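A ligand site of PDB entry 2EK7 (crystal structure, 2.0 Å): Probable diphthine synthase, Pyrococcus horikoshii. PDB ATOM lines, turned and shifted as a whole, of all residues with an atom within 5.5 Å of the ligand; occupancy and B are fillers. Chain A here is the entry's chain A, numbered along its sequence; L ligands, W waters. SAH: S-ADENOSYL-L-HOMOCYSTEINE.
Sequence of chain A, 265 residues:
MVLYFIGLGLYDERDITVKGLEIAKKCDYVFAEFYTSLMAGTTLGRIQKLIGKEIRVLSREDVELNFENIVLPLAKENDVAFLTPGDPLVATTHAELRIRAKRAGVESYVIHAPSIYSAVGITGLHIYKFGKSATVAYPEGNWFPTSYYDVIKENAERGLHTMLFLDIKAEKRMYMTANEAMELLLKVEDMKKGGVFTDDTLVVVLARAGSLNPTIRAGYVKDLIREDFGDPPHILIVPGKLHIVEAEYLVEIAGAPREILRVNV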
ATOM      1  N   LEU A  10      24.810   4.334 -25.116  1.00  0.00           N
ATOM      2  CA  LEU A  10      24.996   5.733 -24.739  1.00  0.00           C
ATOM      3  C   LEU A  10      26.314   6.315 -24.252  1.00  0.00           C
ATOM      4  O   LEU A  10      26.736   7.373 -24.744  1.00  0.00           O
ATOM      5  CB  LEU A  10      23.967   6.079 -23.677  1.00  0.00           C
ATOM      6  CG  LEU A  10      22.478   5.938 -23.983  1.00  0.00           C
ATOM      7  CD1 LEU A  10      21.707   6.068 -22.679  1.00  0.00           C
ATOM      8  CD2 LEU A  10      22.049   6.993 -24.999  1.00  0.00           C
ATOM      9  N   TYR A  11      26.940   5.661 -23.289  1.00  0.00           N
ATOM     10  CA  TYR A  11      28.137   6.226 -22.661  1.00  0.00           C
ATOM     11  C   TYR A  11      29.429   5.413 -22.616  1.00  0.00           C
ATOM     12  O   TYR A  11      30.489   5.915 -22.987  1.00  0.00           O
ATOM     13  CB  TYR A  11      27.727   6.644 -21.245  1.00  0.00           C
ATOM     14  CG  TYR A  11      28.769   7.394 -20.463  1.00  0.00           C
ATOM     15  CD1 TYR A  11      29.165   8.690 -20.830  1.00  0.00           C
ATOM     16  CD2 TYR A  11      29.359   6.837 -19.328  1.00  0.00           C
ATOM     17  CE1 TYR A  11      30.112   9.398 -20.096  1.00  0.00           C
ATOM     18  CE2 TYR A  11      30.308   7.528 -18.580  1.00  0.00           C
ATOM     19  CZ  TYR A  11      30.672   8.804 -18.975  1.00  0.00           C
ATOM     20  OH  TYR A  11      31.614   9.483 -18.234  1.00  0.00           O
ATOM     21  N   THR A  36      29.527   9.118 -35.704  1.00  0.00           N
ATOM     22  CA  THR A  36      28.121   9.521 -35.590  1.00  0.00           C
ATOM     23  C   THR A  36      27.748   9.987 -34.190  1.00  0.00           C
ATOM     24  O   THR A  36      26.702  10.608 -33.988  1.00  0.00           O
ATOM     25  CB  THR A  36      27.163   8.369 -35.991  1.00  0.00           C
ATOM     26  OG1 THR A  36      27.464   7.188 -35.239  1.00  0.00           O
ATOM     27  CG2 THR A  36      27.282   8.080 -37.481  1.00  0.00           C
ATOM     28  N   SER A  37      28.580   9.673 -33.211  1.00  0.00           N
ATOM     29  CA  SER A  37      28.285  10.092 -31.852  1.00  0.00           C
ATOM     30  C   SER A  37      29.524   9.951 -30.981  1.00  0.00           C
ATOM     31  O   SER A  37      30.575   9.500 -31.449  1.00  0.00           O
ATOM     32  CB  SER A  37      27.151   9.255 -31.269  1.00  0.00           C
ATOM     33  OG  SER A  37      26.766   9.743 -29.997  1.00  0.00           O
ATOM     34  N   LEU A  38      29.393  10.335 -29.719  1.00  0.00           N
ATOM     35  CA  LEU A  38      30.508  10.239 -28.801  1.00  0.00           C
ATOM     36  C   LEU A  38      30.140   9.422 -27.571  1.00  0.00           C
ATOM     37  O   LEU A  38      29.129   9.673 -26.920  1.00  0.00           O
ATOM     38  CB  LEU A  38      30.960  11.641 -28.371  1.00  0.00           C
ATOM     39  CG  LEU A  38      32.033  11.730 -27.281  1.00  0.00           C
ATOM     40  CD1 LEU A  38      33.334  11.093 -27.776  1.00  0.00           C
ATOM     41  CD2 LEU A  38      32.261  13.177 -26.906  1.00  0.00           C
ATOM     42  N   PRO A  85      28.074   3.816 -32.002  1.00  0.00           N
ATOM     43  CA  PRO A  85      27.655   4.336 -30.695  1.00  0.00           C
ATOM     44  C   PRO A  85      26.121   4.312 -30.684  1.00  0.00           C
ATOM     45  O   PRO A  85      25.501   4.243 -31.742  1.00  0.00           O
ATOM     46  CB  PRO A  85      28.196   5.770 -30.706  1.00  0.00           C
ATOM     47  CG  PRO A  85      29.332   5.713 -31.696  1.00  0.00           C
ATOM     48  CD  PRO A  85      28.810   4.824 -32.779  1.00  0.00           C
ATOM     49  N   GLY A  86      25.527   4.358 -29.492  1.00  0.00           N
ATOM     50  CA  GLY A  86      24.071   4.353 -29.370  1.00  0.00           C
ATOM     51  C   GLY A  86      23.403   3.243 -30.161  1.00  0.00           C
ATOM     52  O   GLY A  86      23.875   2.101 -30.149  1.00  0.00           O
ATOM     53  N   ASP A  87      22.289   3.569 -30.823  1.00  0.00           N
ATOM     54  CA  ASP A  87      21.592   2.585 -31.657  1.00  0.00           C
ATOM     55  C   ASP A  87      22.085   2.861 -33.067  1.00  0.00           C
ATOM     56  O   ASP A  87      22.079   4.006 -33.526  1.00  0.00           O
ATOM     57  CB  ASP A  87      20.077   2.755 -31.582  1.00  0.00           C
ATOM     58  CG  ASP A  87      19.336   1.747 -32.456  1.00  0.00           C
ATOM     59  OD1 ASP A  87      19.399   1.874 -33.705  1.00  0.00           O
ATOM     60  OD2 ASP A  87      18.707   0.821 -31.892  1.00  0.00           O
ATOM     61  N   PRO A  88      22.520   1.813 -33.779  1.00  0.00           N
ATOM     62  CA  PRO A  88      23.030   1.925 -35.144  1.00  0.00           C
ATOM     63  C   PRO A  88      22.190   2.631 -36.202  1.00  0.00           C
ATOM     64  O   PRO A  88      22.752   3.224 -37.134  1.00  0.00           O
ATOM     65  CB  PRO A  88      23.346   0.478 -35.508  1.00  0.00           C
ATOM     66  CG  PRO A  88      22.357  -0.304 -34.708  1.00  0.00           C
ATOM     67  CD  PRO A  88      22.375   0.395 -33.385  1.00  0.00           C
ATOM     68  N   LEU A  89      20.874   2.600 -36.066  1.00  0.00           N
ATOM     69  CA  LEU A  89      20.011   3.208 -37.070  1.00  0.00           C
ATOM     70  C   LEU A  89      19.374   4.540 -36.688  1.00  0.00           C
ATOM     71  O   LEU A  89      18.645   5.118 -37.490  1.00  0.00           O
ATOM     72  CB  LEU A  89      18.917   2.220 -37.471  1.00  0.00           C
ATOM     73  CG  LEU A  89      19.417   0.827 -37.881  1.00  0.00           C
ATOM     74  CD1 LEU A  89      18.223  -0.023 -38.296  1.00  0.00           C
ATOM     75  CD2 LEU A  89      20.408   0.939 -39.024  1.00  0.00           C
ATOM     76  N   VAL A  90      19.637   5.021 -35.482  1.00  0.00           N
ATOM     77  CA  VAL A  90      19.048   6.265 -35.030  1.00  0.00           C
ATOM     78  C   VAL A  90      19.889   7.495 -35.367  1.00  0.00           C
ATOM     79  O   VAL A  90      21.054   7.607 -34.993  1.00  0.00           O
ATOM     80  CB  VAL A  90      18.814   6.228 -33.501  1.00  0.00           C
ATOM     81  CG1 VAL A  90      18.341   7.581 -32.997  1.00  0.00           C
ATOM     82  CG2 VAL A  90      17.794   5.149 -33.174  1.00  0.00           C
ATOM     83  N   ALA A  91      19.284   8.431 -36.106  1.00  0.00           N
ATOM     84  CA  ALA A  91      19.949   9.667 -36.500  1.00  0.00           C
ATOM     85  C   ALA A  91      21.262   9.418 -37.229  1.00  0.00           C
ATOM     86  O   ALA A  91      22.235  10.151 -37.049  1.00  0.00           O
ATOM     87  CB  ALA A  91      20.183  10.562 -35.269  1.00  0.00           C
ATOM     88  N   THR A  92      21.298   8.358 -38.019  1.00  0.00           N
ATOM     89  CA  THR A  92      22.426   8.025 -38.865  1.00  0.00           C
ATOM     90  C   THR A  92      21.832   7.642 -40.179  1.00  0.00           C
ATOM     91  O   THR A  92      20.618   7.580 -40.313  1.00  0.00           O
ATOM     92  CB  THR A  92      23.215   6.815 -38.287  1.00  0.00           C
ATOM     93  OG1 THR A  92      22.460   5.621 -38.479  1.00  0.00           O
ATOM     94  CG2 THR A  92      23.543   6.981 -36.801  1.00  0.00           C
ATOM     95  N   PRO A 114      20.767   1.116 -26.064  1.00  0.00           N
ATOM     96  CA  PRO A 114      20.124   2.360 -25.633  1.00  0.00           C
ATOM     97  C   PRO A 114      20.505   3.538 -26.535  1.00  0.00           C
ATOM     98  O   PRO A 114      21.672   3.705 -26.914  1.00  0.00           O
ATOM     99  CB  PRO A 114      20.598   2.530 -24.176  1.00  0.00           C
ATOM    100  CG  PRO A 114      21.673   1.515 -23.875  1.00  0.00           C
ATOM    101  CD  PRO A 114      21.519   0.493 -24.967  1.00  0.00           C
ATOM    102  N   SER A 115      19.508   4.344 -26.887  1.00  0.00           N
ATOM    103  CA  SER A 115      19.684   5.494 -27.765  1.00  0.00           C
ATOM    104  C   SER A 115      19.331   6.784 -27.050  1.00  0.00           C
ATOM    105  O   SER A 115      18.482   6.799 -26.158  1.00  0.00           O
ATOM    106  CB  SER A 115      18.772   5.341 -28.982  1.00  0.00           C
ATOM    107  OG  SER A 115      18.762   6.524 -29.764  1.00  0.00           O
ATOM    108  N   ILE A 116      19.986   7.871 -27.464  1.00  0.00           N
ATOM    109  CA  ILE A 116      19.700   9.163 -26.851  1.00  0.00           C
ATOM    110  C   ILE A 116      18.231   9.518 -27.120  1.00  0.00           C
ATOM    111  O   ILE A 116      17.595  10.206 -26.322  1.00  0.00           O
ATOM    112  CB  ILE A 116      20.633  10.280 -27.415  1.00  0.00           C
ATOM    113  CG1 ILE A 116      20.385  11.588 -26.672  1.00  0.00           C
ATOM    114  CG2 ILE A 116      20.395  10.471 -28.916  1.00  0.00           C
ATOM    115  CD1 ILE A 116      20.720  11.521 -25.194  1.00  0.00           C
ATOM    116  N   TYR A 117      17.686   9.014 -28.218  1.00  0.00           N
ATOM    117  CA  TYR A 117      16.312   9.304 -28.587  1.00  0.00           C
ATOM    118  C   TYR A 117      15.286   8.879 -27.525  1.00  0.00           C
ATOM    119  O   TYR A 117      14.261   9.533 -27.344  1.00  0.00           O
ATOM    120  CB  TYR A 117      15.964   8.661 -29.939  1.00  0.00           C
ATOM    121  CG  TYR A 117      14.663   9.165 -30.533  1.00  0.00           C
ATOM    122  CD1 TYR A 117      14.572  10.470 -31.031  1.00  0.00           C
ATOM    123  CD2 TYR A 117      13.532   8.352 -30.594  1.00  0.00           C
ATOM    124  CE1 TYR A 117      13.374  10.946 -31.577  1.00  0.00           C
ATOM    125  CE2 TYR A 117      12.339   8.821 -31.134  1.00  0.00           C
ATOM    126  CZ  TYR A 117      12.262  10.124 -31.629  1.00  0.00           C
ATOM    127  OH  TYR A 117      11.089  10.581 -32.169  1.00  0.00           O
ATOM    128  N   LEU A 164      16.794  18.383 -29.992  1.00  0.00           N
ATOM    129  CA  LEU A 164      17.797  18.865 -30.925  1.00  0.00           C
ATOM    130  C   LEU A 164      19.119  18.121 -30.788  1.00  0.00           C
ATOM    131  O   LEU A 164      19.836  18.276 -29.799  1.00  0.00           O
ATOM    132  CB  LEU A 164      18.049  20.366 -30.695  1.00  0.00           C
ATOM    133  CG  LEU A 164      16.837  21.307 -30.780  1.00  0.00           C
ATOM    134  CD1 LEU A 164      17.201  22.697 -30.258  1.00  0.00           C
ATOM    135  CD2 LEU A 164      16.363  21.380 -32.223  1.00  0.00           C
ATOM    136  N   PHE A 165      19.436  17.295 -31.784  1.00  0.00           N
ATOM    137  CA  PHE A 165      20.701  16.579 -31.798  1.00  0.00           C
ATOM    138  C   PHE A 165      21.708  17.691 -32.052  1.00  0.00           C
ATOM    139  O   PHE A 165      21.381  18.664 -32.749  1.00  0.00           O
ATOM    140  CB  PHE A 165      20.749  15.585 -32.966  1.00  0.00           C
ATOM    141  CG  PHE A 165      19.804  14.423 -32.815  1.00  0.00           C
ATOM    142  CD1 PHE A 165      20.172  13.322 -32.035  1.00  0.00           C
ATOM    143  CD2 PHE A 165      18.560  14.430 -33.433  1.00  0.00           C
ATOM    144  CE1 PHE A 165      19.308  12.245 -31.882  1.00  0.00           C
ATOM    145  CE2 PHE A 165      17.682  13.354 -33.283  1.00  0.00           C
ATOM    146  CZ  PHE A 165      18.053  12.265 -32.510  1.00  0.00           C
ATOM    147  N   LEU A 166      22.905  17.575 -31.501  1.00  0.00           N
ATOM    148  CA  LEU A 166      23.914  18.611 -31.700  1.00  0.00           C
ATOM    149  C   LEU A 166      25.029  18.125 -32.626  1.00  0.00           C
ATOM    150  O   LEU A 166      25.361  16.940 -32.655  1.00  0.00           O
ATOM    151  CB  LEU A 166      24.461  19.067 -30.346  1.00  0.00           C
ATOM    152  CG  LEU A 166      23.391  19.599 -29.372  1.00  0.00           C
ATOM    153  CD1 LEU A 166      24.059  20.263 -28.170  1.00  0.00           C
ATOM    154  CD2 LEU A 166      22.498  20.620 -30.092  1.00  0.00           C
ATOM    155  N   ASP A 167      25.613  19.059 -33.375  1.00  0.00           N
ATOM    156  CA  ASP A 167      26.644  18.733 -34.340  1.00  0.00           C
ATOM    157  C   ASP A 167      27.889  18.055 -33.769  1.00  0.00           C
ATOM    158  O   ASP A 167      28.199  18.155 -32.584  1.00  0.00           O
ATOM    159  CB  ASP A 167      27.056  19.998 -35.114  1.00  0.00           C
ATOM    160  CG  ASP A 167      27.508  19.687 -36.537  1.00  0.00           C
ATOM    161  OD1 ASP A 167      27.621  18.497 -36.891  1.00  0.00           O
ATOM    162  OD2 ASP A 167      27.735  20.644 -37.309  1.00  0.00           O
ATOM    163  N   ILE A 168      28.595  17.351 -34.655  1.00  0.00           N
ATOM    164  CA  ILE A 168      29.819  16.652 -34.293  1.00  0.00           C
ATOM    165  C   ILE A 168      30.781  16.599 -35.473  1.00  0.00           C
ATOM    166  O   ILE A 168      30.386  16.291 -36.599  1.00  0.00           O
ATOM    167  CB  ILE A 168      29.507  15.212 -33.812  1.00  0.00           C
ATOM    168  CG1 ILE A 168      30.800  14.450 -33.556  1.00  0.00           C
ATOM    169  CG2 ILE A 168      28.656  14.491 -34.843  1.00  0.00           C
ATOM    170  CD1 ILE A 168      30.590  13.040 -33.031  1.00  0.00           C
ATOM    171  N   LEU A 206      20.604  17.894 -21.530  1.00  0.00           N
ATOM    172  CA  LEU A 206      20.926  16.546 -21.076  1.00  0.00           C
ATOM    173  C   LEU A 206      22.329  16.253 -21.575  1.00  0.00           C
ATOM    174  O   LEU A 206      22.582  16.240 -22.795  1.00  0.00           O
ATOM    175  CB  LEU A 206      19.919  15.537 -21.646  1.00  0.00           C
ATOM    176  CG  LEU A 206      20.187  14.048 -21.397  1.00  0.00           C
ATOM    177  CD1 LEU A 206      20.421  13.776 -19.914  1.00  0.00           C
ATOM    178  CD2 LEU A 206      18.990  13.241 -21.905  1.00  0.00           C
ATOM    179  N   ALA A 207      23.257  16.053 -20.649  1.00  0.00           N
ATOM    180  CA  ALA A 207      24.638  15.776 -21.015  1.00  0.00           C
ATOM    181  C   ALA A 207      25.108  14.430 -20.503  1.00  0.00           C
ATOM    182  O   ALA A 207      24.849  14.063 -19.362  1.00  0.00           O
ATOM    183  CB  ALA A 207      25.545  16.876 -20.476  1.00  0.00           C
ATOM    184  N   ARG A 208      25.794  13.704 -21.377  1.00  0.00           N
ATOM    185  CA  ARG A 208      26.346  12.396 -21.050  1.00  0.00           C
ATOM    186  C   ARG A 208      25.328  11.387 -20.513  1.00  0.00           C
ATOM    187  O   ARG A 208      25.564  10.727 -19.497  1.00  0.00           O
ATOM    188  CB  ARG A 208      27.500  12.567 -20.054  1.00  0.00           C
ATOM    189  CG  ARG A 208      28.588  13.545 -20.533  1.00  0.00           C
ATOM    190  CD  ARG A 208      29.677  13.744 -19.494  1.00  0.00           C
ATOM    191  NE  ARG A 208      29.114  14.121 -18.196  1.00  0.00           N
ATOM    192  CZ  ARG A 208      28.566  15.297 -17.923  1.00  0.00           C
ATOM    193  NH1 ARG A 208      28.494  16.240 -18.855  1.00  0.00           N
ATOM    194  NH2 ARG A 208      28.055  15.526 -16.724  1.00  0.00           N
ATOM    195  N   ALA A 209      24.192  11.286 -21.199  1.00  0.00           N
ATOM    196  CA  ALA A 209      23.181  10.321 -20.802  1.00  0.00           C
ATOM    197  C   ALA A 209      23.883   8.968 -20.865  1.00  0.00           C
ATOM    198  O   ALA A 209      24.751   8.747 -21.707  1.00  0.00           O
ATOM    199  CB  ALA A 209      22.002  10.355 -21.786  1.00  0.00           C
ATOM    200  N   GLY A 210      23.522   8.050 -19.969  1.00  0.00           N
ATOM    201  CA  GLY A 210      24.162   6.748 -19.965  1.00  0.00           C
ATOM    202  C   GLY A 210      25.150   6.651 -18.808  1.00  0.00           C
ATOM    203  O   GLY A 210      25.403   5.569 -18.280  1.00  0.00           O
ATOM    204  N   PRO A 233      28.966  14.233 -24.885  1.00  0.00           N
ATOM    205  CA  PRO A 233      27.974  14.878 -25.751  1.00  0.00           C
ATOM    206  C   PRO A 233      26.804  15.513 -25.000  1.00  0.00           C
ATOM    207  O   PRO A 233      26.494  15.128 -23.867  1.00  0.00           O
ATOM    208  CB  PRO A 233      27.533  13.738 -26.658  1.00  0.00           C
ATOM    209  CG  PRO A 233      27.514  12.583 -25.703  1.00  0.00           C
ATOM    210  CD  PRO A 233      28.814  12.769 -24.929  1.00  0.00           C
ATOM    211  N   HIS A 234      26.160  16.474 -25.652  1.00  0.00           N
ATOM    212  CA  HIS A 234      24.996  17.172 -25.091  1.00  0.00           C
ATOM    213  C   HIS A 234      23.869  17.144 -26.110  1.00  0.00           C
ATOM    214  O   HIS A 234      24.103  17.050 -27.313  1.00  0.00           O
ATOM    215  CB  HIS A 234      25.272  18.665 -24.877  1.00  0.00           C
ATOM    216  CG  HIS A 234      26.385  18.981 -23.927  1.00  0.00           C
ATOM    217  ND1 HIS A 234      26.760  20.284 -23.650  1.00  0.00           N
ATOM    218  CD2 HIS A 234      27.183  18.194 -23.165  1.00  0.00           C
ATOM    219  CE1 HIS A 234      27.735  20.271 -22.750  1.00  0.00           C
ATOM    220  NE2 HIS A 234      28.006  19.019 -22.445  1.00  0.00           N
ATOM    221  N   ILE A 235      22.648  17.274 -25.616  1.00  0.00           N
ATOM    222  CA  ILE A 235      21.503  17.430 -26.507  1.00  0.00           C
ATOM    223  C   ILE A 235      20.739  18.570 -25.874  1.00  0.00           C
ATOM    224  O   ILE A 235      20.771  18.747 -24.652  1.00  0.00           O
ATOM    225  CB  ILE A 235      20.561  16.199 -26.591  1.00  0.00           C
ATOM    226  CG1 ILE A 235      20.081  15.794 -25.200  1.00  0.00           C
ATOM    227  CG2 ILE A 235      21.251  15.063 -27.312  1.00  0.00           C
ATOM    228  CD1 ILE A 235      18.811  14.934 -25.251  1.00  0.00           C
HETATM  229  N   SAH L   1      22.632   6.623 -33.133  1.00  0.00           N
HETATM  230  CA  SAH L   1      22.876   7.584 -31.983  1.00  0.00           C
HETATM  231  CB  SAH L   1      22.683   9.037 -32.257  1.00  0.00           C
HETATM  232  CG  SAH L   1      23.490   9.676 -33.380  1.00  0.00           C
HETATM  233  SD  SAH L   1      23.271  11.498 -33.276  1.00  0.00           S
HETATM  234  C   SAH L   1      21.949   7.098 -30.778  1.00  0.00           C
HETATM  235  O   SAH L   1      21.213   6.117 -30.955  1.00  0.00           O
HETATM  236  OXT SAH L   1      22.025   7.775 -29.689  1.00  0.00           O
HETATM  237  C5' SAH L   1      24.569  11.896 -32.171  1.00  0.00           C
HETATM  238  C4' SAH L   1      24.162  13.146 -31.301  1.00  0.00           C
HETATM  239  O4' SAH L   1      23.149  12.700 -30.370  1.00  0.00           O
HETATM  240  C3' SAH L   1      25.256  13.746 -30.492  1.00  0.00           C
HETATM  241  O3' SAH L   1      25.955  14.727 -31.244  1.00  0.00           O
HETATM  242  C2' SAH L   1      24.487  14.289 -29.269  1.00  0.00           C
HETATM  243  O2' SAH L   1      23.916  15.586 -29.516  1.00  0.00           O
HETATM  244  C1' SAH L   1      23.440  13.191 -28.995  1.00  0.00           C
HETATM  245  N9  SAH L   1      23.872  12.194 -28.191  1.00  0.00           N
HETATM  246  C8  SAH L   1      24.304  10.883 -28.398  1.00  0.00           C
HETATM  247  N7  SAH L   1      24.620  10.237 -27.317  1.00  0.00           N
HETATM  248  C5  SAH L   1      24.394  11.158 -26.262  1.00  0.00           C
HETATM  249  C6  SAH L   1      24.553  11.045 -24.828  1.00  0.00           C
HETATM  250  N6  SAH L   1      24.978   9.938 -24.206  1.00  0.00           N
HETATM  251  N1  SAH L   1      24.222  12.176 -24.121  1.00  0.00           N
HETATM  252  C2  SAH L   1      23.784  13.324 -24.700  1.00  0.00           C
HETATM  253  N3  SAH L   1      23.612  13.471 -26.061  1.00  0.00           N
HETATM  254  C4  SAH L   1      23.945  12.351 -26.775  1.00  0.00           C
HETATM  255  O   HOH W   1      24.372   7.421 -28.052  1.00  0.00           O
HETATM  256  O   HOH W   2      25.441   6.416 -33.534  1.00  0.00           O
HETATM  257  O   HOH W   3      28.198  16.132 -30.328  1.00  0.00           O
HETATM  258  O   HOH W   4      26.937   7.875 -28.044  1.00  0.00           O
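The side-chain carboxylate of Asp 87 lies within hydrogen-bond range of the backbone NH of Leu 89.
N of Tyr 117 lies close to OG of Ser 115, at 3.1 Å.
The backbone NH (N) of Ile 235 is in hydrogen-bond range of the backbone carbonyl oxygen (O) of Leu 206 (3.0 Å).
N of Arg 208 is in hydrogen-bond range of O of Pro 233.
The side-chain hydroxyl (OG1) of Thr 92 lies within hydrogen-bond range of the backbone carbonyl oxygen (O) of Pro 88 (2.8 Å).
The backbone carbonyl oxygen (O) of Val 90 is in hydrogen-bond range of a nitrogen (N) of the ligand (2.6 Å).
An oxygen (O2') of the ligand sits at hydrogen-bond distance from the backbone carbonyl oxygen (O) of His 234, at 2.7 Å.
N of Leu 166 sits at hydrogen-bond distance from O2' of the ligand (3.0 Å).
The backbone carbonyl oxygen (O) of Leu 166 is in hydrogen-bond range of an oxygen (O3') of the ligand, 2.7 Å away.
The backbone NH (N) of Asp 87 lies within hydrogen-bond range of an oxygen (O) of the ligand (2.8 Å).
O of Asp 87 lies within hydrogen-bond range of N of the ligand.
The side-chain hydroxyl (OG) of Ser 115 sits at hydrogen-bond distance from an oxygen (O) of the ligand (2.8 Å).
N of Ala 209 is in hydrogen-bond range of N1 of the ligand (3.1 Å).
The backbone carbonyl oxygen (O) of Ala 209 lies within hydrogen-bond range of a nitrogen (N6) of the ligand (2.8 Å).
OXT of the ligand is in hydrogen-bond range of N of Ile 116, at 3.0 Å.
The side-chain hydroxyl of Ser 37 lies close to a nitrogen (N7) of the ligand (3.5 Å).
A nitrogen (N6) of the ligand lies within hydrogen-bond range of the backbone carbonyl oxygen (O) of Leu 10 (3.2 Å).
Water W3 bridges O3' of the ligand (2.8 Å) and O of Asp 167 (3.0 Å).
Water W2 lies within hydrogen-bond range of OG1 of Thr 36, O of Pro 85 and N of the ligand.
The backbone carbonyl oxygen (O) of Thr 36 sits close to a sulfur (SD) of the ligand, at 3.6 Å.
O of Pro 85 touches N of the ligand, at 3.98 Å.
C of Gly 86 touches O of the ligand, at 3.7 Å.
CB of Ala 91 touches SD of the ligand (3.8 Å).
CG2 of Thr 92 touches N of the ligand (3.8 Å).
Phe 165 touches the ligand (CD1 to O4', 3.5 Å).
O of Leu 206 touches C2 of the ligand (3.7 Å).
N of Arg 208 touches N1 of the ligand, 3.5 Å away.
Pro 233 touches the ligand (O to C2, 3.4 Å).
CG2 of Ile 235 touches N3 of the ligand (3.1 Å).
Hydrophobic or aromatic side chains that line the ligand: Val 90, Ala 91, Ile 116, Phe 165, Leu 166, Ala 209, Pro 233 and Ile 235.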
